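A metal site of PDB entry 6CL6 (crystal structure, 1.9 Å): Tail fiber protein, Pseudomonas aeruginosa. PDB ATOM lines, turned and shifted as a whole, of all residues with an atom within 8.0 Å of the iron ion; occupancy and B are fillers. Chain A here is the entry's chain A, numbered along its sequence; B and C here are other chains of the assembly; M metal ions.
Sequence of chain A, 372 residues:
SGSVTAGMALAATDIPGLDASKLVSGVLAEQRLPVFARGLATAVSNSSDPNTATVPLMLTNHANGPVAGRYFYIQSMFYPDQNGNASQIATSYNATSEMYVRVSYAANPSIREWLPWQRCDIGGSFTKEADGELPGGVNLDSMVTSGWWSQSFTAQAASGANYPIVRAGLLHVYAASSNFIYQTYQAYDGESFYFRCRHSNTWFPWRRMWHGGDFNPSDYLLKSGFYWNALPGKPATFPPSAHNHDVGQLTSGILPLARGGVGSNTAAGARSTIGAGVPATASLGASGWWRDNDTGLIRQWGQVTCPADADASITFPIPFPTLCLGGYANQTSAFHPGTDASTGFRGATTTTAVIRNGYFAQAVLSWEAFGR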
ATOM      1  N   PRO A 240       4.408  24.444  -5.013  1.00  0.00           N
ATOM      2  CA  PRO A 240       4.475  23.810  -3.689  1.00  0.00           C
ATOM      3  C   PRO A 240       5.597  22.797  -3.580  1.00  0.00           C
ATOM      4  O   PRO A 240       6.024  22.178  -4.555  1.00  0.00           O
ATOM      5  CB  PRO A 240       3.099  23.137  -3.553  1.00  0.00           C
ATOM      6  CG  PRO A 240       2.722  22.813  -4.957  1.00  0.00           C
ATOM      7  CD  PRO A 240       3.311  23.890  -5.830  1.00  0.00           C
ATOM      8  N   SER A 241       6.047  22.599  -2.347  1.00  0.00           N
ATOM      9  CA  SER A 241       6.917  21.481  -2.026  1.00  0.00           C
ATOM     10  C   SER A 241       6.066  20.226  -1.797  1.00  0.00           C
ATOM     11  O   SER A 241       4.849  20.308  -1.568  1.00  0.00           O
ATOM     12  CB  SER A 241       7.762  21.808  -0.800  1.00  0.00           C
ATOM     13  OG  SER A 241       6.969  22.198   0.305  1.00  0.00           O
ATOM     14  N   ALA A 242       6.706  19.075  -1.866  1.00  0.00           N
ATOM     15  CA  ALA A 242       5.969  17.804  -1.796  1.00  0.00           C
ATOM     16  C   ALA A 242       5.121  17.727  -0.536  1.00  0.00           C
ATOM     17  O   ALA A 242       5.554  18.091   0.569  1.00  0.00           O
ATOM     18  CB  ALA A 242       6.963  16.635  -1.840  1.00  0.00           C
ATOM     19  N   HIS A 243       3.889  17.240  -0.700  1.00  0.00           N
ATOM     20  CA  HIS A 243       2.951  17.170   0.406  1.00  0.00           C
ATOM     21  C   HIS A 243       1.935  16.061   0.152  1.00  0.00           C
ATOM     22  O   HIS A 243       1.714  15.637  -0.980  1.00  0.00           O
ATOM     23  CB  HIS A 243       2.217  18.512   0.609  1.00  0.00           C
ATOM     24  CG  HIS A 243       1.459  18.963  -0.603  1.00  0.00           C
ATOM     25  ND1 HIS A 243       2.080  19.490  -1.706  1.00  0.00           N
ATOM     26  CD2 HIS A 243       0.135  18.953  -0.883  1.00  0.00           C
ATOM     27  CE1 HIS A 243       1.172  19.792  -2.618  1.00  0.00           C
ATOM     28  NE2 HIS A 243      -0.016  19.468  -2.148  1.00  0.00           N
ATOM     29  N   ASN A 244       1.322  15.603   1.218  1.00  0.00           N
ATOM     30  CA  ASN A 244       0.251  14.615   1.131  1.00  0.00           C
ATOM     31  C   ASN A 244      -1.100  15.294   1.310  1.00  0.00           C
ATOM     32  O   ASN A 244      -1.192  16.501   1.557  1.00  0.00           O
ATOM     33  CB  ASN A 244       0.484  13.519   2.176  1.00  0.00           C
ATOM     34  CG  ASN A 244       1.714  12.710   1.882  1.00  0.00           C
ATOM     35  OD1 ASN A 244       2.052  12.466   0.730  1.00  0.00           O
ATOM     36  ND2 ASN A 244       2.410  12.272   2.943  1.00  0.00           N
ATOM     37  N   HIS A 245      -2.160  14.510   1.198  1.00  0.00           N
ATOM     38  CA  HIS A 245      -3.512  15.047   1.296  1.00  0.00           C
ATOM     39  C   HIS A 245      -4.419  14.029   1.961  1.00  0.00           C
ATOM     40  O   HIS A 245      -4.179  12.815   1.914  1.00  0.00           O
ATOM     41  CB  HIS A 245      -4.102  15.383  -0.084  1.00  0.00           C
ATOM     42  CG  HIS A 245      -3.738  16.742  -0.598  1.00  0.00           C
ATOM     43  ND1 HIS A 245      -4.196  17.894   0.009  1.00  0.00           N
ATOM     44  CD2 HIS A 245      -2.976  17.137  -1.639  1.00  0.00           C
ATOM     45  CE1 HIS A 245      -3.724  18.939  -0.654  1.00  0.00           C
ATOM     46  NE2 HIS A 245      -2.983  18.501  -1.658  1.00  0.00           N
ATOM     47  N   GLN A 249      -9.990  16.564   0.941  1.00  0.00           N
ATOM     48  CA  GLN A 249      -9.600  17.714   0.137  1.00  0.00           C
ATOM     49  C   GLN A 249      -9.852  17.511  -1.349  1.00  0.00           C
ATOM     50  O   GLN A 249      -9.599  18.414  -2.142  1.00  0.00           O
ATOM     51  CB  GLN A 249      -8.137  18.041   0.381  1.00  0.00           C
ATOM     52  CG  GLN A 249      -7.907  18.900   1.614  1.00  0.00           C
ATOM     53  CD  GLN A 249      -7.061  18.206   2.658  1.00  0.00           C
ATOM     54  OE1 GLN A 249      -5.899  17.835   2.404  1.00  0.00           O
ATOM     55  NE2 GLN A 249      -7.634  18.014   3.856  1.00  0.00           N
ATOM     56  N   PRO B 240      -0.626  27.441  -2.841  1.00  0.00           N
ATOM     57  CA  PRO B 240       0.086  26.726  -3.909  1.00  0.00           C
ATOM     58  C   PRO B 240      -0.492  27.031  -5.279  1.00  0.00           C
ATOM     59  O   PRO B 240      -1.691  27.251  -5.442  1.00  0.00           O
ATOM     60  CB  PRO B 240      -0.118  25.243  -3.542  1.00  0.00           C
ATOM     61  CG  PRO B 240      -1.430  25.233  -2.822  1.00  0.00           C
ATOM     62  CD  PRO B 240      -1.476  26.529  -2.037  1.00  0.00           C
ATOM     63  N   SER B 241       0.398  27.027  -6.271  1.00  0.00           N
ATOM     64  CA  SER B 241      -0.025  27.084  -7.657  1.00  0.00           C
ATOM     65  C   SER B 241      -0.518  25.708  -8.112  1.00  0.00           C
ATOM     66  O   SER B 241      -0.379  24.717  -7.399  1.00  0.00           O
ATOM     67  CB  SER B 241       1.101  27.604  -8.521  1.00  0.00           C
ATOM     68  OG  SER B 241       2.306  26.921  -8.233  1.00  0.00           O
ATOM     69  N   ALA B 242      -1.078  25.656  -9.322  1.00  0.00           N
ATOM     70  CA  ALA B 242      -1.701  24.425  -9.805  1.00  0.00           C
ATOM     71  C   ALA B 242      -0.683  23.294  -9.922  1.00  0.00           C
ATOM     72  O   ALA B 242       0.376  23.450 -10.536  1.00  0.00           O
ATOM     73  CB  ALA B 242      -2.364  24.673 -11.164  1.00  0.00           C
ATOM     74  N   HIS B 243      -1.025  22.137  -9.352  1.00  0.00           N
ATOM     75  CA  HIS B 243      -0.118  21.006  -9.391  1.00  0.00           C
ATOM     76  C   HIS B 243      -0.893  19.688  -9.461  1.00  0.00           C
ATOM     77  O   HIS B 243      -2.071  19.598  -9.106  1.00  0.00           O
ATOM     78  CB  HIS B 243       0.812  20.999  -8.182  1.00  0.00           C
ATOM     79  CG  HIS B 243       0.070  21.008  -6.868  1.00  0.00           C
ATOM     80  ND1 HIS B 243      -0.638  22.095  -6.417  1.00  0.00           N
ATOM     81  CD2 HIS B 243      -0.025  20.068  -5.897  1.00  0.00           C
ATOM     82  CE1 HIS B 243      -1.148  21.822  -5.228  1.00  0.00           C
ATOM     83  NE2 HIS B 243      -0.805  20.598  -4.899  1.00  0.00           N
ATOM     84  N   ASN B 244      -0.202  18.654  -9.904  1.00  0.00           N
ATOM     85  CA  ASN B 244      -0.710  17.292 -10.005  1.00  0.00           C
ATOM     86  C   ASN B 244      -0.209  16.459  -8.835  1.00  0.00           C
ATOM     87  O   ASN B 244       0.754  16.801  -8.150  1.00  0.00           O
ATOM     88  CB  ASN B 244      -0.284  16.667 -11.327  1.00  0.00           C
ATOM     89  CG  ASN B 244      -0.999  17.287 -12.507  1.00  0.00           C
ATOM     90  OD1 ASN B 244      -2.143  17.740 -12.388  1.00  0.00           O
ATOM     91  ND2 ASN B 244      -0.342  17.302 -13.659  1.00  0.00           N
ATOM     92  N   HIS B 245      -0.898  15.343  -8.599  1.00  0.00           N
ATOM     93  CA  HIS B 245      -0.557  14.445  -7.493  1.00  0.00           C
ATOM     94  C   HIS B 245      -0.623  13.001  -7.948  1.00  0.00           C
ATOM     95  O   HIS B 245      -1.379  12.641  -8.853  1.00  0.00           O
ATOM     96  CB  HIS B 245      -1.521  14.614  -6.317  1.00  0.00           C
ATOM     97  CG  HIS B 245      -1.184  15.727  -5.386  1.00  0.00           C
ATOM     98  ND1 HIS B 245      -0.172  15.628  -4.454  1.00  0.00           N
ATOM     99  CD2 HIS B 245      -1.749  16.953  -5.212  1.00  0.00           C
ATOM    100  CE1 HIS B 245      -0.114  16.757  -3.755  1.00  0.00           C
ATOM    101  NE2 HIS B 245      -1.064  17.562  -4.187  1.00  0.00           N
ATOM    102  N   GLN B 249      -0.058   9.845  -2.644  1.00  0.00           N
ATOM    103  CA  GLN B 249       0.030  10.960  -1.699  1.00  0.00           C
ATOM    104  C   GLN B 249      -1.277  11.222  -0.964  1.00  0.00           C
ATOM    105  O   GLN B 249      -1.313  12.125  -0.101  1.00  0.00           O
ATOM    106  CB  GLN B 249       0.490  12.214  -2.444  1.00  0.00           C
ATOM    107  CG  GLN B 249       1.979  12.202  -2.717  1.00  0.00           C
ATOM    108  CD  GLN B 249       2.395  13.291  -3.664  1.00  0.00           C
ATOM    109  OE1 GLN B 249       1.671  13.619  -4.604  1.00  0.00           O
ATOM    110  NE2 GLN B 249       3.550  13.895  -3.402  1.00  0.00           N
ATOM    111  N   PRO C 240       3.037  24.421   1.131  1.00  0.00           N
ATOM    112  CA  PRO C 240       1.715  24.912   0.755  1.00  0.00           C
ATOM    113  C   PRO C 240       0.800  25.087   1.950  1.00  0.00           C
ATOM    114  O   PRO C 240       0.918  24.381   2.959  1.00  0.00           O
ATOM    115  CB  PRO C 240       1.181  23.832  -0.192  1.00  0.00           C
ATOM    116  CG  PRO C 240       1.770  22.588   0.356  1.00  0.00           C
ATOM    117  CD  PRO C 240       3.173  22.975   0.830  1.00  0.00           C
ATOM    118  N   SER C 241      -0.089  26.060   1.835  1.00  0.00           N
ATOM    119  CA  SER C 241      -1.190  26.201   2.766  1.00  0.00           C
ATOM    120  C   SER C 241      -2.287  25.193   2.402  1.00  0.00           C
ATOM    121  O   SER C 241      -2.243  24.554   1.357  1.00  0.00           O
ATOM    122  CB  SER C 241      -1.738  27.631   2.739  1.00  0.00           C
ATOM    123  OG  SER C 241      -2.027  28.044   1.425  1.00  0.00           O
ATOM    124  N   ALA C 242      -3.270  25.053   3.276  1.00  0.00           N
ATOM    125  CA  ALA C 242      -4.343  24.090   3.047  1.00  0.00           C
ATOM    126  C   ALA C 242      -5.064  24.435   1.743  1.00  0.00           C
ATOM    127  O   ALA C 242      -5.360  25.595   1.458  1.00  0.00           O
ATOM    128  CB  ALA C 242      -5.331  24.099   4.221  1.00  0.00           C
ATOM    129  N   HIS C 243      -5.319  23.415   0.940  1.00  0.00           N
ATOM    130  CA  HIS C 243      -5.960  23.623  -0.350  1.00  0.00           C
ATOM    131  C   HIS C 243      -6.696  22.356  -0.743  1.00  0.00           C
ATOM    132  O   HIS C 243      -6.475  21.284  -0.186  1.00  0.00           O
ATOM    133  CB  HIS C 243      -4.940  24.023  -1.417  1.00  0.00           C
ATOM    134  CG  HIS C 243      -3.867  23.008  -1.629  1.00  0.00           C
ATOM    135  ND1 HIS C 243      -2.885  22.730  -0.690  1.00  0.00           N
ATOM    136  CD2 HIS C 243      -3.622  22.175  -2.679  1.00  0.00           C
ATOM    137  CE1 HIS C 243      -2.083  21.786  -1.155  1.00  0.00           C
ATOM    138  NE2 HIS C 243      -2.505  21.435  -2.357  1.00  0.00           N
ATOM    139  N   ASN C 244      -7.561  22.492  -1.744  1.00  0.00           N
ATOM    140  CA  ASN C 244      -8.372  21.406  -2.272  1.00  0.00           C
ATOM    141  C   ASN C 244      -7.966  21.114  -3.706  1.00  0.00           C
ATOM    142  O   ASN C 244      -7.311  21.929  -4.366  1.00  0.00           O
ATOM    143  CB  ASN C 244      -9.853  21.755  -2.215  1.00  0.00           C
ATOM    144  CG  ASN C 244     -10.362  21.865  -0.796  1.00  0.00           C
ATOM    145  OD1 ASN C 244      -9.871  21.176   0.101  1.00  0.00           O
ATOM    146  ND2 ASN C 244     -11.311  22.763  -0.578  1.00  0.00           N
ATOM    147  N   HIS C 245      -8.362  19.938  -4.181  1.00  0.00           N
ATOM    148  CA  HIS C 245      -8.044  19.492  -5.520  1.00  0.00           C
ATOM    149  C   HIS C 245      -9.278  18.947  -6.217  1.00  0.00           C
ATOM    150  O   HIS C 245     -10.174  18.386  -5.576  1.00  0.00           O
ATOM    151  CB  HIS C 245      -6.965  18.398  -5.517  1.00  0.00           C
ATOM    152  CG  HIS C 245      -5.580  18.915  -5.371  1.00  0.00           C
ATOM    153  ND1 HIS C 245      -4.926  19.577  -6.396  1.00  0.00           N
ATOM    154  CD2 HIS C 245      -4.701  18.872  -4.340  1.00  0.00           C
ATOM    155  CE1 HIS C 245      -3.714  19.917  -5.994  1.00  0.00           C
ATOM    156  NE2 HIS C 245      -3.555  19.502  -4.749  1.00  0.00           N
ATOM    157  N   GLN C 249      -6.549  16.439 -11.137  1.00  0.00           N
ATOM    158  CA  GLN C 249      -5.128  16.602 -10.847  1.00  0.00           C
ATOM    159  C   GLN C 249      -4.506  15.356 -10.222  1.00  0.00           C
ATOM    160  O   GLN C 249      -3.318  15.371  -9.898  1.00  0.00           O
ATOM    161  CB  GLN C 249      -4.892  17.807  -9.925  1.00  0.00           C
ATOM    162  CG  GLN C 249      -5.100  19.156 -10.587  1.00  0.00           C
ATOM    163  CD  GLN C 249      -6.375  19.839 -10.140  1.00  0.00           C
ATOM    164  OE1 GLN C 249      -6.572  20.138  -8.953  1.00  0.00           O
ATOM    165  NE2 GLN C 249      -7.272  20.082 -11.092  1.00  0.00           N
HETATM  166 FE    FE M   1      -1.861  19.480  -3.286  1.00  0.00          FE
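The iron ion is bound by a ring nitrogen (NE2) of His 243 of chain A (2.2 Å), a ring nitrogen (NE2) of His 245 of chain A (2.2 Å), a ring nitrogen (NE2) of His 243 of chain B (2.2 Å), a ring nitrogen (NE2) of His 245 of chain C (2.2 Å), a ring nitrogen (NE2) of His 243 of chain C (2.3 Å) and a ring nitrogen (NE2) of His 245 of chain B (2.3 Å). The iron ion has six donor atoms within binding distance.
Of the 21 residues printed, 6 come within 4 Å of the iron ion. Along chain A the residues within 4 Å of the iron ion span positions 243 to 245. The nearest printed residue that does not touch the iron ion is Asn 244 of chain A (5.7 Å).
The backbone carbonyl oxygen (O) of Ser 241 of chain A sits at hydrogen-bond distance from a ring nitrogen (ND1) of His 243 of chain A (2.9 Å). The side-chain amide oxygen (OE1) of Gln 249 of chain A sits at hydrogen-bond distance from a ring nitrogen (ND1) of His 245 of chain A (2.9 Å). A ring nitrogen (ND1) of His 243 of chain B sits at hydrogen-bond distance from the backbone carbonyl oxygen (O) of Ser 241 of chain B (2.8 Å). The backbone NH (N) of His 245 of chain C sits at hydrogen-bond distance from the backbone carbonyl oxygen (O) of Gln 249 of chain A (2.8 Å). The side-chain amide oxygen of Gln 249 of chain C is in hydrogen-bond range of a ring nitrogen (ND1) of His 245 of chain C. A ring nitrogen (ND1) of His 243 of chain C lies within hydrogen-bond range of the backbone carbonyl oxygen of Ser 241 of chain C (2.8 Å). A ring nitrogen (ND1) of His 245 of chain B sits at hydrogen-bond distance from the side-chain amide oxygen (OE1) of Gln 249 of chain B (2.7 Å). The backbone NH (N) of His 245 of chain B lies within hydrogen-bond range of the backbone carbonyl oxygen (O) of Gln 249 of chain C, 2.7 Å away.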
